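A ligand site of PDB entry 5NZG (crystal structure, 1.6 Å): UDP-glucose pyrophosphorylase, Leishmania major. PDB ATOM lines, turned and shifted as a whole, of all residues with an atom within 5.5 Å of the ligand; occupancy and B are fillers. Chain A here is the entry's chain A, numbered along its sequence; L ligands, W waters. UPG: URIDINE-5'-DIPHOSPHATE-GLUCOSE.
The side-chain carboxylate (OE2) of Glu 284 sits at hydrogen-bond distance from an oxygen (O2') of the ligand, at 2.5 Å.
O4' of the ligand is in hydrogen-bond range of O of Asn 306, at 2.7 Å.
O3' of the ligand is in hydrogen-bond range of ND2 of Asn 306 (2.8 Å).
O2B of the ligand sits at hydrogen-bond distance from NE2 of His 191 (2.7 Å).
The side-chain amino group (NZ) of Lys 380 is in salt-bridge range of an oxygen (O2A) of the ligand.
An oxygen (O2C) of the ligand lies within hydrogen-bond range of the backbone NH of Gly 84.
The backbone NH (N) of Gly 83 is in hydrogen-bond range of an oxygen (O2) of the ligand (2.9 Å).
OE1 of Gln 162 lies within hydrogen-bond range of N3 of the ligand, at 2.9 Å.
N of Gly 257 sits at hydrogen-bond distance from O4' of the ligand (3.0 Å).
O of Gly 257 sits at hydrogen-bond distance from O4' of the ligand (3.4 Å).
ND2 of Asn 219 is in hydrogen-bond range of O5' of the ligand (3.1 Å).
The backbone NH of Gly 220 sits at hydrogen-bond distance from an oxygen (O3C) of the ligand (3.2 Å).
N of Gly 190 sits close to O4 of the ligand, 3.3 Å away.
O3C of the ligand is in hydrogen-bond range of O of Leu 81 (3.2 Å).
The backbone NH of Asn 306 sits at hydrogen-bond distance from the backbone carbonyl oxygen of Gly 257 (2.9 Å).
OD1 of Asn 306 sits at hydrogen-bond distance from N of Asn 308 (2.8 Å).
The side-chain carboxylate of Asp 221 lies within salt-bridge range of the side-chain amino group of Lys 380, at 3.0 Å.
NE2 of Gln 162 sits at hydrogen-bond distance from O of Gly 83, at 3.3 Å.
The backbone NH (N) of Gly 83 sits at hydrogen-bond distance from the backbone carbonyl oxygen (O) of Met 130, 3.1 Å away.
O of Leu 81 lies within hydrogen-bond range of N of Gly 220 (3.1 Å).
N of Asn 82 sits at hydrogen-bond distance from O of Met 130, at 2.8 Å.
The backbone NH (N) of Val 379 is in hydrogen-bond range of the side-chain carboxylate (OD2) of Asp 221 (3.0 Å).
Residues that only touch the ligand: Pro 188 (3.3 Å), Gly 256 (3.4 Å), Met 130 (3.5 Å), Phe 305 (3.5 Å), Asn 308 (3.6 Å), Phe 376 (3.7 Å), Asp 221 (3.7 Å), Asn 82 (3.7 Å), Leu 282 (3.7 Å) and Thr 307 (3.96 Å).
Hydrophobic or aromatic side chains that line the ligand: Leu 81, Met 130, Pro 188, His 191, Leu 282, Phe 305 and Phe 376.
Within 4 Å of the ligand: Leu 81, Asn 82, Gly 83, Gly 84, Met 130, Gln 162, Pro 188, Gly 190, His 191, Asn 219, Gly 220, Asp 221, Gly 256, Gly 257, Leu 282, Glu 284, Phe 305, Asn 306, Thr 307, Asn 308, Phe 376 and Lys 380.
The nearest printed residue that does not touch the ligand is Pro 378 (4.01 Å).
Water W12 lies within hydrogen-bond range of O2A of the ligand (2.6 Å), NZ of Lys 95 (2.8 Å) and OD1 of Asp 221 (2.9 Å).
Water W4 bridges O6' of the ligand (2.7 Å) and O of Lys 255 (2.8 Å).
Water W13 lies within hydrogen-bond range of the side-chain amide oxygen (OD1) of Asn 308, an oxygen (O2') of the ligand and the side-chain amide nitrogen (ND2) of Asn 306.
Water W6 lies within hydrogen-bond range of O1B of the ligand (2.8 Å), OE2 of Glu 284 (2.9 Å) and O of Gly 256 (3.3 Å).
Water W5 lies within hydrogen-bond range of OD2 of Asp 221, O6' of the ligand, ND2 of Asn 219 and NZ of Lys 380.
Water W8 lies within hydrogen-bond range of the side-chain carboxylate of Glu 284 and an oxygen (O2B) of the ligand.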
ATOM      1  N   LEU A  81     -24.710   1.875  -3.028  1.00  0.00           N
ATOM      2  CA  LEU A  81     -25.174   3.120  -3.619  1.00  0.00           C
ATOM      3  C   LEU A  81     -24.194   3.596  -4.682  1.00  0.00           C
ATOM      4  O   LEU A  81     -22.971   3.539  -4.488  1.00  0.00           O
ATOM      5  CB  LEU A  81     -25.351   4.187  -2.534  1.00  0.00           C
ATOM      6  CG  LEU A  81     -26.271   3.833  -1.362  1.00  0.00           C
ATOM      7  CD1 LEU A  81     -26.199   4.918  -0.300  1.00  0.00           C
ATOM      8  CD2 LEU A  81     -27.700   3.625  -1.826  1.00  0.00           C
ATOM      9  N   ASN A  82     -24.731   4.074  -5.798  1.00  0.00           N
ATOM     10  CA  ASN A  82     -23.897   4.426  -6.948  1.00  0.00           C
ATOM     11  C   ASN A  82     -24.599   5.415  -7.867  1.00  0.00           C
ATOM     12  O   ASN A  82     -24.362   5.422  -9.077  1.00  0.00           O
ATOM     13  CB  ASN A  82     -23.509   3.154  -7.706  1.00  0.00           C
ATOM     14  CG  ASN A  82     -22.344   3.365  -8.653  1.00  0.00           C
ATOM     15  OD1 ASN A  82     -21.354   4.017  -8.311  1.00  0.00           O
ATOM     16  ND2 ASN A  82     -22.453   2.818  -9.862  1.00  0.00           N
ATOM     17  N   GLY A  83     -25.472   6.245  -7.309  1.00  0.00           N
ATOM     18  CA  GLY A  83     -26.252   7.146  -8.129  1.00  0.00           C
ATOM     19  C   GLY A  83     -25.929   8.618  -7.944  1.00  0.00           C
ATOM     20  O   GLY A  83     -26.540   9.474  -8.583  1.00  0.00           O
ATOM     21  N   GLY A  84     -24.968   8.914  -7.080  1.00  0.00           N
ATOM     22  CA  GLY A  84     -24.615  10.296  -6.809  1.00  0.00           C
ATOM     23  C   GLY A  84     -23.711  10.893  -7.861  1.00  0.00           C
ATOM     24  O   GLY A  84     -23.116  10.213  -8.692  1.00  0.00           O
ATOM     25  N   LEU A  85     -23.609  12.223  -7.814  1.00  0.00           N
ATOM     26  CA  LEU A  85     -22.727  12.988  -8.697  1.00  0.00           C
ATOM     27  C   LEU A  85     -21.792  13.809  -7.810  1.00  0.00           C
ATOM     28  O   LEU A  85     -22.192  14.831  -7.253  1.00  0.00           O
ATOM     29  CB  LEU A  85     -23.522  13.883  -9.639  1.00  0.00           C
ATOM     30  CG  LEU A  85     -23.457  13.498 -11.120  1.00  0.00           C
ATOM     31  CD1 LEU A  85     -23.911  12.065 -11.306  1.00  0.00           C
ATOM     32  CD2 LEU A  85     -24.277  14.454 -11.971  1.00  0.00           C
ATOM     33  N   LYS A  95     -18.397   8.135  -9.240  1.00  0.00           N
ATOM     34  CA  LYS A  95     -17.170   8.194  -8.441  1.00  0.00           C
ATOM     35  C   LYS A  95     -16.502   6.835  -8.338  1.00  0.00           C
ATOM     36  O   LYS A  95     -15.268   6.754  -8.230  1.00  0.00           O
ATOM     37  CB  LYS A  95     -17.475   8.754  -7.048  1.00  0.00           C
ATOM     38  CG  LYS A  95     -16.280   8.834  -6.123  1.00  0.00           C
ATOM     39  CD  LYS A  95     -16.707   9.197  -4.708  1.00  0.00           C
ATOM     40  CE  LYS A  95     -17.176  10.639  -4.629  1.00  0.00           C
ATOM     41  NZ  LYS A  95     -17.667  10.977  -3.267  1.00  0.00           N
ATOM     42  N   MET A 130     -27.514   0.628  -6.843  1.00  0.00           N
ATOM     43  CA  MET A 130     -28.482   1.682  -7.118  1.00  0.00           C
ATOM     44  C   MET A 130     -27.805   2.755  -7.967  1.00  0.00           C
ATOM     45  O   MET A 130     -26.931   3.481  -7.478  1.00  0.00           O
ATOM     46  CB  MET A 130     -29.057   2.295  -5.842  1.00  0.00           C
ATOM     47  CG  MET A 130     -30.086   3.376  -6.151  1.00  0.00           C
ATOM     48  SD  MET A 130     -31.003   3.983  -4.736  1.00  0.00           S
ATOM     49  CE  MET A 130     -30.074   5.463  -4.331  1.00  0.00           C
ATOM     50  N   GLN A 162     -32.584   4.653  -9.553  1.00  0.00           N
ATOM     51  CA  GLN A 162     -33.191   5.630  -8.654  1.00  0.00           C
ATOM     52  C   GLN A 162     -34.120   6.557  -9.436  1.00  0.00           C
ATOM     53  O   GLN A 162     -34.022   6.690 -10.663  1.00  0.00           O
ATOM     54  CB  GLN A 162     -32.117   6.432  -7.935  1.00  0.00           C
ATOM     55  CG  GLN A 162     -31.276   7.313  -8.829  1.00  0.00           C
ATOM     56  CD  GLN A 162     -30.229   8.097  -8.062  1.00  0.00           C
ATOM     57  OE1 GLN A 162     -29.742   7.646  -7.022  1.00  0.00           O
ATOM     58  NE2 GLN A 162     -29.873   9.268  -8.574  1.00  0.00           N
ATOM     59  N   PRO A 188     -31.841  13.955  -8.734  1.00  0.00           N
ATOM     60  CA  PRO A 188     -31.997  12.814  -7.837  1.00  0.00           C
ATOM     61  C   PRO A 188     -32.515  13.262  -6.487  1.00  0.00           C
ATOM     62  O   PRO A 188     -32.188  14.365  -6.017  1.00  0.00           O
ATOM     63  CB  PRO A 188     -30.562  12.257  -7.738  1.00  0.00           C
ATOM     64  CG  PRO A 188     -29.846  12.800  -8.936  1.00  0.00           C
ATOM     65  CD  PRO A 188     -30.450  14.140  -9.174  1.00  0.00           C
ATOM     66  N   PRO A 189     -33.328  12.441  -5.828  1.00  0.00           N
ATOM     67  CA  PRO A 189     -33.895  12.849  -4.534  1.00  0.00           C
ATOM     68  C   PRO A 189     -33.074  12.344  -3.358  1.00  0.00           C
ATOM     69  O   PRO A 189     -33.631  12.083  -2.282  1.00  0.00           O
ATOM     70  CB  PRO A 189     -35.293  12.211  -4.550  1.00  0.00           C
ATOM     71  CG  PRO A 189     -35.303  11.234  -5.737  1.00  0.00           C
ATOM     72  CD  PRO A 189     -33.909  11.182  -6.297  1.00  0.00           C
ATOM     73  N   GLY A 190     -31.769  12.207  -3.534  1.00  0.00           N
ATOM     74  CA  GLY A 190     -30.900  11.697  -2.481  1.00  0.00           C
ATOM     75  C   GLY A 190     -30.941  10.182  -2.386  1.00  0.00           C
ATOM     76  O   GLY A 190     -31.791   9.516  -2.988  1.00  0.00           O
ATOM     77  N   HIS A 191     -30.008   9.633  -1.605  1.00  0.00           N
ATOM     78  CA  HIS A 191     -29.945   8.181  -1.473  1.00  0.00           C
ATOM     79  C   HIS A 191     -31.040   7.625  -0.561  1.00  0.00           C
ATOM     80  O   HIS A 191     -31.205   6.405  -0.498  1.00  0.00           O
ATOM     81  CB  HIS A 191     -28.574   7.737  -0.959  1.00  0.00           C
ATOM     82  CG  HIS A 191     -28.048   8.552   0.180  1.00  0.00           C
ATOM     83  ND1 HIS A 191     -28.636   8.574   1.424  1.00  0.00           N
ATOM     84  CD2 HIS A 191     -26.960   9.369   0.263  1.00  0.00           C
ATOM     85  CE1 HIS A 191     -27.943   9.366   2.221  1.00  0.00           C
ATOM     86  NE2 HIS A 191     -26.927   9.854   1.544  1.00  0.00           N
ATOM     87  N   ASN A 219     -22.314   2.946   1.225  1.00  0.00           N
ATOM     88  CA  ASN A 219     -21.901   3.881   0.188  1.00  0.00           C
ATOM     89  C   ASN A 219     -20.955   3.212  -0.792  1.00  0.00           C
ATOM     90  O   ASN A 219     -20.150   2.343  -0.433  1.00  0.00           O
ATOM     91  CB  ASN A 219     -21.215   5.098   0.810  1.00  0.00           C
ATOM     92  CG  ASN A 219     -22.157   5.917   1.672  1.00  0.00           C
ATOM     93  OD1 ASN A 219     -23.372   5.888   1.495  1.00  0.00           O
ATOM     94  ND2 ASN A 219     -21.603   6.667   2.618  1.00  0.00           N
ATOM     95  N   GLY A 220     -21.051   3.627  -2.061  1.00  0.00           N
ATOM     96  CA  GLY A 220     -20.132   3.124  -3.064  1.00  0.00           C
ATOM     97  C   GLY A 220     -18.693   3.538  -2.842  1.00  0.00           C
ATOM     98  O   GLY A 220     -17.781   2.861  -3.336  1.00  0.00           O
ATOM     99  N   ASP A 221     -18.473   4.623  -2.108  1.00  0.00           N
ATOM    100  CA  ASP A 221     -17.131   5.125  -1.849  1.00  0.00           C
ATOM    101  C   ASP A 221     -16.486   4.483  -0.620  1.00  0.00           C
ATOM    102  O   ASP A 221     -15.300   4.736  -0.366  1.00  0.00           O
ATOM    103  CB  ASP A 221     -17.154   6.646  -1.668  1.00  0.00           C
ATOM    104  CG  ASP A 221     -17.969   7.077  -0.465  1.00  0.00           C
ATOM    105  OD1 ASP A 221     -19.195   7.286  -0.614  1.00  0.00           O
ATOM    106  OD2 ASP A 221     -17.392   7.207   0.635  1.00  0.00           O
ATOM    107  N   LYS A 255     -17.998  15.731   6.550  1.00  0.00           N
ATOM    108  CA  LYS A 255     -19.071  15.704   5.570  1.00  0.00           C
ATOM    109  C   LYS A 255     -19.866  14.421   5.750  1.00  0.00           C
ATOM    110  O   LYS A 255     -19.344  13.324   5.523  1.00  0.00           O
ATOM    111  CB  LYS A 255     -18.522  15.838   4.149  1.00  0.00           C
ATOM    112  CG  LYS A 255     -17.561  17.004   3.996  1.00  0.00           C
ATOM    113  CD  LYS A 255     -16.949  17.048   2.601  1.00  0.00           C
ATOM    114  CE  LYS A 255     -17.849  17.790   1.637  1.00  0.00           C
ATOM    115  NZ  LYS A 255     -17.866  19.256   1.900  1.00  0.00           N
ATOM    116  N   GLY A 256     -21.113  14.553   6.146  1.00  0.00           N
ATOM    117  CA  GLY A 256     -21.975  13.426   6.414  1.00  0.00           C
ATOM    118  C   GLY A 256     -23.011  13.802   7.472  1.00  0.00           C
ATOM    119  O   GLY A 256     -23.487  14.940   7.492  1.00  0.00           O
ATOM    120  N   GLY A 257     -23.332  12.834   8.329  1.00  0.00           N
ATOM    121  CA  GLY A 257     -24.292  13.055   9.380  1.00  0.00           C
ATOM    122  C   GLY A 257     -23.892  12.321  10.641  1.00  0.00           C
ATOM    123  O   GLY A 257     -23.116  11.357  10.611  1.00  0.00           O
ATOM    124  N   HIS A 258     -24.441  12.786  11.762  1.00  0.00           N
ATOM    125  CA  HIS A 258     -24.170  12.202  13.070  1.00  0.00           C
ATOM    126  C   HIS A 258     -25.465  11.698  13.691  1.00  0.00           C
ATOM    127  O   HIS A 258     -26.570  12.153  13.365  1.00  0.00           O
ATOM    128  CB  HIS A 258     -23.495  13.212  14.004  1.00  0.00           C
ATOM    129  CG  HIS A 258     -24.372  14.370  14.392  1.00  0.00           C
ATOM    130  ND1 HIS A 258     -25.366  14.276  15.333  1.00  0.00           N
ATOM    131  CD2 HIS A 258     -24.387  15.653  13.957  1.00  0.00           C
ATOM    132  CE1 HIS A 258     -25.974  15.445  15.463  1.00  0.00           C
ATOM    133  NE2 HIS A 258     -25.389  16.298  14.641  1.00  0.00           N
ATOM    134  N   LEU A 282     -31.120  10.805  12.575  1.00  0.00           N
ATOM    135  CA  LEU A 282     -29.927  11.246  11.856  1.00  0.00           C
ATOM    136  C   LEU A 282     -30.029  12.734  11.547  1.00  0.00           C
ATOM    137  O   LEU A 282     -31.113  13.220  11.206  1.00  0.00           O
ATOM    138  CB  LEU A 282     -29.754  10.449  10.560  1.00  0.00           C
ATOM    139  CG  LEU A 282     -28.658  10.886   9.590  1.00  0.00           C
ATOM    140  CD1 LEU A 282     -27.287  10.505  10.113  1.00  0.00           C
ATOM    141  CD2 LEU A 282     -28.886  10.305   8.207  1.00  0.00           C
ATOM    142  N   GLU A 284     -28.029  15.223   9.057  1.00  0.00           N
ATOM    143  CA  GLU A 284     -27.025  15.535   8.059  1.00  0.00           C
ATOM    144  C   GLU A 284     -26.504  16.955   8.271  1.00  0.00           C
ATOM    145  O   GLU A 284     -27.108  17.759   8.981  1.00  0.00           O
ATOM    146  CB  GLU A 284     -27.609  15.391   6.642  1.00  0.00           C
ATOM    147  CG  GLU A 284     -28.079  13.987   6.310  1.00  0.00           C
ATOM    148  CD  GLU A 284     -26.935  13.011   6.177  1.00  0.00           C
ATOM    149  OE1 GLU A 284     -26.583  12.375   7.192  1.00  0.00           O
ATOM    150  OE2 GLU A 284     -26.386  12.877   5.069  1.00  0.00           O
ATOM    151  N   PHE A 305     -20.649   9.115  14.377  1.00  0.00           N
ATOM    152  CA  PHE A 305     -20.756   9.482  12.980  1.00  0.00           C
ATOM    153  C   PHE A 305     -21.365   8.331  12.194  1.00  0.00           C
ATOM    154  O   PHE A 305     -20.911   7.187  12.295  1.00  0.00           O
ATOM    155  CB  PHE A 305     -19.381   9.844  12.416  1.00  0.00           C
ATOM    156  CG  PHE A 305     -19.436  10.765  11.226  1.00  0.00           C
ATOM    157  CD1 PHE A 305     -19.841  12.081  11.364  1.00  0.00           C
ATOM    158  CD2 PHE A 305     -19.067  10.312   9.970  1.00  0.00           C
ATOM    159  CE1 PHE A 305     -19.886  12.936  10.275  1.00  0.00           C
ATOM    160  CE2 PHE A 305     -19.108  11.159   8.870  1.00  0.00           C
ATOM    161  CZ  PHE A 305     -19.513  12.472   9.028  1.00  0.00           C
ATOM    162  N   ASN A 306     -22.391   8.633  11.407  1.00  0.00           N
ATOM    163  CA  ASN A 306     -23.026   7.621  10.573  1.00  0.00           C
ATOM    164  C   ASN A 306     -22.069   7.169   9.475  1.00  0.00           C
ATOM    165  O   ASN A 306     -21.501   7.999   8.752  1.00  0.00           O
ATOM    166  CB  ASN A 306     -24.319   8.151   9.970  1.00  0.00           C
ATOM    167  CG  ASN A 306     -24.988   7.153   9.038  1.00  0.00           C
ATOM    168  OD1 ASN A 306     -24.885   5.943   9.229  1.00  0.00           O
ATOM    169  ND2 ASN A 306     -25.679   7.669   8.013  1.00  0.00           N
ATOM    170  N   THR A 307     -21.869   5.861   9.364  1.00  0.00           N
ATOM    171  CA  THR A 307     -21.073   5.294   8.292  1.00  0.00           C
ATOM    172  C   THR A 307     -21.875   5.035   7.025  1.00  0.00           C
ATOM    173  O   THR A 307     -21.276   4.815   5.963  1.00  0.00           O
ATOM    174  CB  THR A 307     -20.430   3.976   8.736  1.00  0.00           C
ATOM    175  OG1 THR A 307     -21.450   2.975   8.875  1.00  0.00           O
ATOM    176  CG2 THR A 307     -19.716   4.150  10.062  1.00  0.00           C
ATOM    177  N   ASN A 308     -23.203   5.093   7.118  1.00  0.00           N
ATOM    178  CA  ASN A 308     -24.128   4.680   6.062  1.00  0.00           C
ATOM    179  C   ASN A 308     -24.018   3.194   5.733  1.00  0.00           C
ATOM    180  O   ASN A 308     -24.467   2.759   4.672  1.00  0.00           O
ATOM    181  CB  ASN A 308     -23.965   5.531   4.796  1.00  0.00           C
ATOM    182  CG  ASN A 308     -25.260   6.202   4.377  1.00  0.00           C
ATOM    183  OD1 ASN A 308     -26.201   6.303   5.166  1.00  0.00           O
ATOM    184  ND2 ASN A 308     -25.312   6.671   3.136  1.00  0.00           N
ATOM    185  N   ALA A 355     -32.197  11.262   3.184  1.00  0.00           N
ATOM    186  CA  ALA A 355     -31.034  10.437   3.470  1.00  0.00           C
ATOM    187  C   ALA A 355     -31.503   9.078   3.965  1.00  0.00           C
ATOM    188  O   ALA A 355     -32.381   8.994   4.834  1.00  0.00           O
ATOM    189  CB  ALA A 355     -30.121  11.096   4.504  1.00  0.00           C
ATOM    190  N   PHE A 376     -15.129   1.633   7.807  1.00  0.00           N
ATOM    191  CA  PHE A 376     -15.500   2.966   7.339  1.00  0.00           C
ATOM    192  C   PHE A 376     -14.251   3.627   6.765  1.00  0.00           C
ATOM    193  O   PHE A 376     -13.378   4.063   7.511  1.00  0.00           O
ATOM    194  CB  PHE A 376     -16.091   3.787   8.487  1.00  0.00           C
ATOM    195  CG  PHE A 376     -16.641   5.113   8.063  1.00  0.00           C
ATOM    196  CD1 PHE A 376     -17.492   5.216   6.976  1.00  0.00           C
ATOM    197  CD2 PHE A 376     -16.316   6.264   8.754  1.00  0.00           C
ATOM    198  CE1 PHE A 376     -18.005   6.432   6.584  1.00  0.00           C
ATOM    199  CE2 PHE A 376     -16.822   7.491   8.374  1.00  0.00           C
ATOM    200  CZ  PHE A 376     -17.666   7.575   7.284  1.00  0.00           C
ATOM    201  N   PRO A 378     -14.289   6.460   4.157  1.00  0.00           N
ATOM    202  CA  PRO A 378     -15.045   7.330   3.250  1.00  0.00           C
ATOM    203  C   PRO A 378     -14.152   8.128   2.322  1.00  0.00           C
ATOM    204  O   PRO A 378     -12.997   8.437   2.626  1.00  0.00           O
ATOM    205  CB  PRO A 378     -15.785   8.258   4.216  1.00  0.00           C
ATOM    206  CG  PRO A 378     -14.870   8.356   5.394  1.00  0.00           C
ATOM    207  CD  PRO A 378     -14.261   6.981   5.535  1.00  0.00           C
ATOM    208  N   VAL A 379     -14.712   8.465   1.163  1.00  0.00           N
ATOM    209  CA  VAL A 379     -14.072   9.352   0.194  1.00  0.00           C
ATOM    210  C   VAL A 379     -15.131  10.376  -0.225  1.00  0.00           C
ATOM    211  O   VAL A 379     -15.927  10.127  -1.146  1.00  0.00           O
ATOM    212  CB  VAL A 379     -13.515   8.604  -1.022  1.00  0.00           C
ATOM    213  CG1 VAL A 379     -12.896   9.582  -2.006  1.00  0.00           C
ATOM    214  CG2 VAL A 379     -12.478   7.580  -0.582  1.00  0.00           C
ATOM    215  N   LYS A 380     -15.154  11.525   0.444  1.00  0.00           N
ATOM    216  CA  LYS A 380     -16.027  12.617   0.082  1.00  0.00           C
ATOM    217  C   LYS A 380     -15.314  13.729  -0.670  1.00  0.00           C
ATOM    218  O   LYS A 380     -15.944  14.441  -1.453  1.00  0.00           O
ATOM    219  CB  LYS A 380     -16.700  13.210   1.327  1.00  0.00           C
ATOM    220  CG  LYS A 380     -17.287  12.175   2.271  1.00  0.00           C
ATOM    221  CD  LYS A 380     -18.549  11.561   1.699  1.00  0.00           C
ATOM    222  CE  LYS A 380     -18.459  10.044   1.699  1.00  0.00           C
ATOM    223  NZ  LYS A 380     -19.762   9.409   1.357  1.00  0.00           N
HETATM  224  N1  UPG L   1     -26.049   8.646  -3.744  1.00  0.00           N
HETATM  225  C2  UPG L   1     -27.016   8.063  -4.582  1.00  0.00           C
HETATM  226  N3  UPG L   1     -28.062   8.899  -5.001  1.00  0.00           N
HETATM  227  C4  UPG L   1     -28.172  10.260  -4.630  1.00  0.00           C
HETATM  228  C5  UPG L   1     -27.127  10.769  -3.765  1.00  0.00           C
HETATM  229  C6  UPG L   1     -26.107   9.976  -3.339  1.00  0.00           C
HETATM  230  O2  UPG L   1     -26.982   6.888  -4.941  1.00  0.00           O
HETATM  231  O4  UPG L   1     -29.125  10.894  -5.063  1.00  0.00           O
HETATM  232  C1C UPG L   1     -24.954   7.756  -3.284  1.00  0.00           C
HETATM  233  C2C UPG L   1     -23.573   8.357  -3.658  1.00  0.00           C
HETATM  234  O2C UPG L   1     -23.264   7.987  -4.960  1.00  0.00           O
HETATM  235  C3C UPG L   1     -22.700   7.653  -2.596  1.00  0.00           C
HETATM  236  C4C UPG L   1     -23.668   7.522  -1.378  1.00  0.00           C
HETATM  237  O4C UPG L   1     -24.989   7.732  -1.869  1.00  0.00           O
HETATM  238  O3C UPG L   1     -22.389   6.356  -2.982  1.00  0.00           O
HETATM  239  C5C UPG L   1     -23.371   8.600  -0.313  1.00  0.00           C
HETATM  240  O5C UPG L   1     -23.555   9.831  -0.862  1.00  0.00           O
HETATM  241  PA  UPG L   1     -22.377  11.060  -0.484  1.00  0.00           P
HETATM  242  O1A UPG L   1     -22.950  12.236  -1.215  1.00  0.00           O
HETATM  243  O2A UPG L   1     -21.078  10.448  -0.856  1.00  0.00           O
HETATM  244  O3A UPG L   1     -22.507  11.257   1.080  1.00  0.00           O
HETATM  245  PB  UPG L   1     -23.577  12.016   1.966  1.00  0.00           P
HETATM  246  O1B UPG L   1     -23.095  13.385   2.334  1.00  0.00           O
HETATM  247  O2B UPG L   1     -24.968  11.727   1.550  1.00  0.00           O
HETATM  248  O3B UPG L   1     -23.450  11.245   3.563  1.00  0.00           O
HETATM  249  C1' UPG L   1     -23.726   9.941   3.697  1.00  0.00           C
HETATM  250  C2' UPG L   1     -24.751   9.770   4.839  1.00  0.00           C
HETATM  251  C3' UPG L   1     -24.138  10.416   6.081  1.00  0.00           C
HETATM  252  C4' UPG L   1     -22.851   9.623   6.440  1.00  0.00           C
HETATM  253  C5' UPG L   1     -21.882   9.664   5.187  1.00  0.00           C
HETATM  254  C6' UPG L   1     -20.703   8.705   5.472  1.00  0.00           C
HETATM  255  O2' UPG L   1     -25.951  10.428   4.568  1.00  0.00           O
HETATM  256  O3' UPG L   1     -24.994  10.279   7.185  1.00  0.00           O
HETATM  257  O4' UPG L   1     -22.181  10.246   7.495  1.00  0.00           O
HETATM  258  O5' UPG L   1     -22.582   9.192   4.066  1.00  0.00           O
HETATM  259  O6' UPG L   1     -19.729   8.916   4.499  1.00  0.00           O
HETATM  260  O   HOH W   1     -20.195   6.567  -4.623  1.00  0.00           O
HETATM  261  O   HOH W   2     -24.196  15.550   0.537  1.00  0.00           O
HETATM  262  O   HOH W   3     -25.775  12.721  -1.169  1.00  0.00           O
HETATM  263  O   HOH W   4     -18.138  10.812   5.510  1.00  0.00           O
HETATM  264  O   HOH W   5     -18.607   6.622   3.003  1.00  0.00           O
HETATM  265  O   HOH W   6     -24.420  14.854   4.341  1.00  0.00           O
HETATM  266  O   HOH W   7     -21.041  10.403  -5.260  1.00  0.00           O
HETATM  267  O   HOH W   8     -27.573  13.488   2.542  1.00  0.00           O
HETATM  268  O   HOH W   9     -23.244  12.076  -3.907  1.00  0.00           O
HETATM  269  O   HOH W  10     -31.760   8.815  -5.541  1.00  0.00           O
HETATM  270  O   HOH W  11     -20.751  14.706   2.029  1.00  0.00           O
HETATM  271  O   HOH W  12     -19.723   9.204  -2.667  1.00  0.00           O
HETATM  272  O   HOH W  13     -27.802   8.530   5.457  1.00  0.00           O
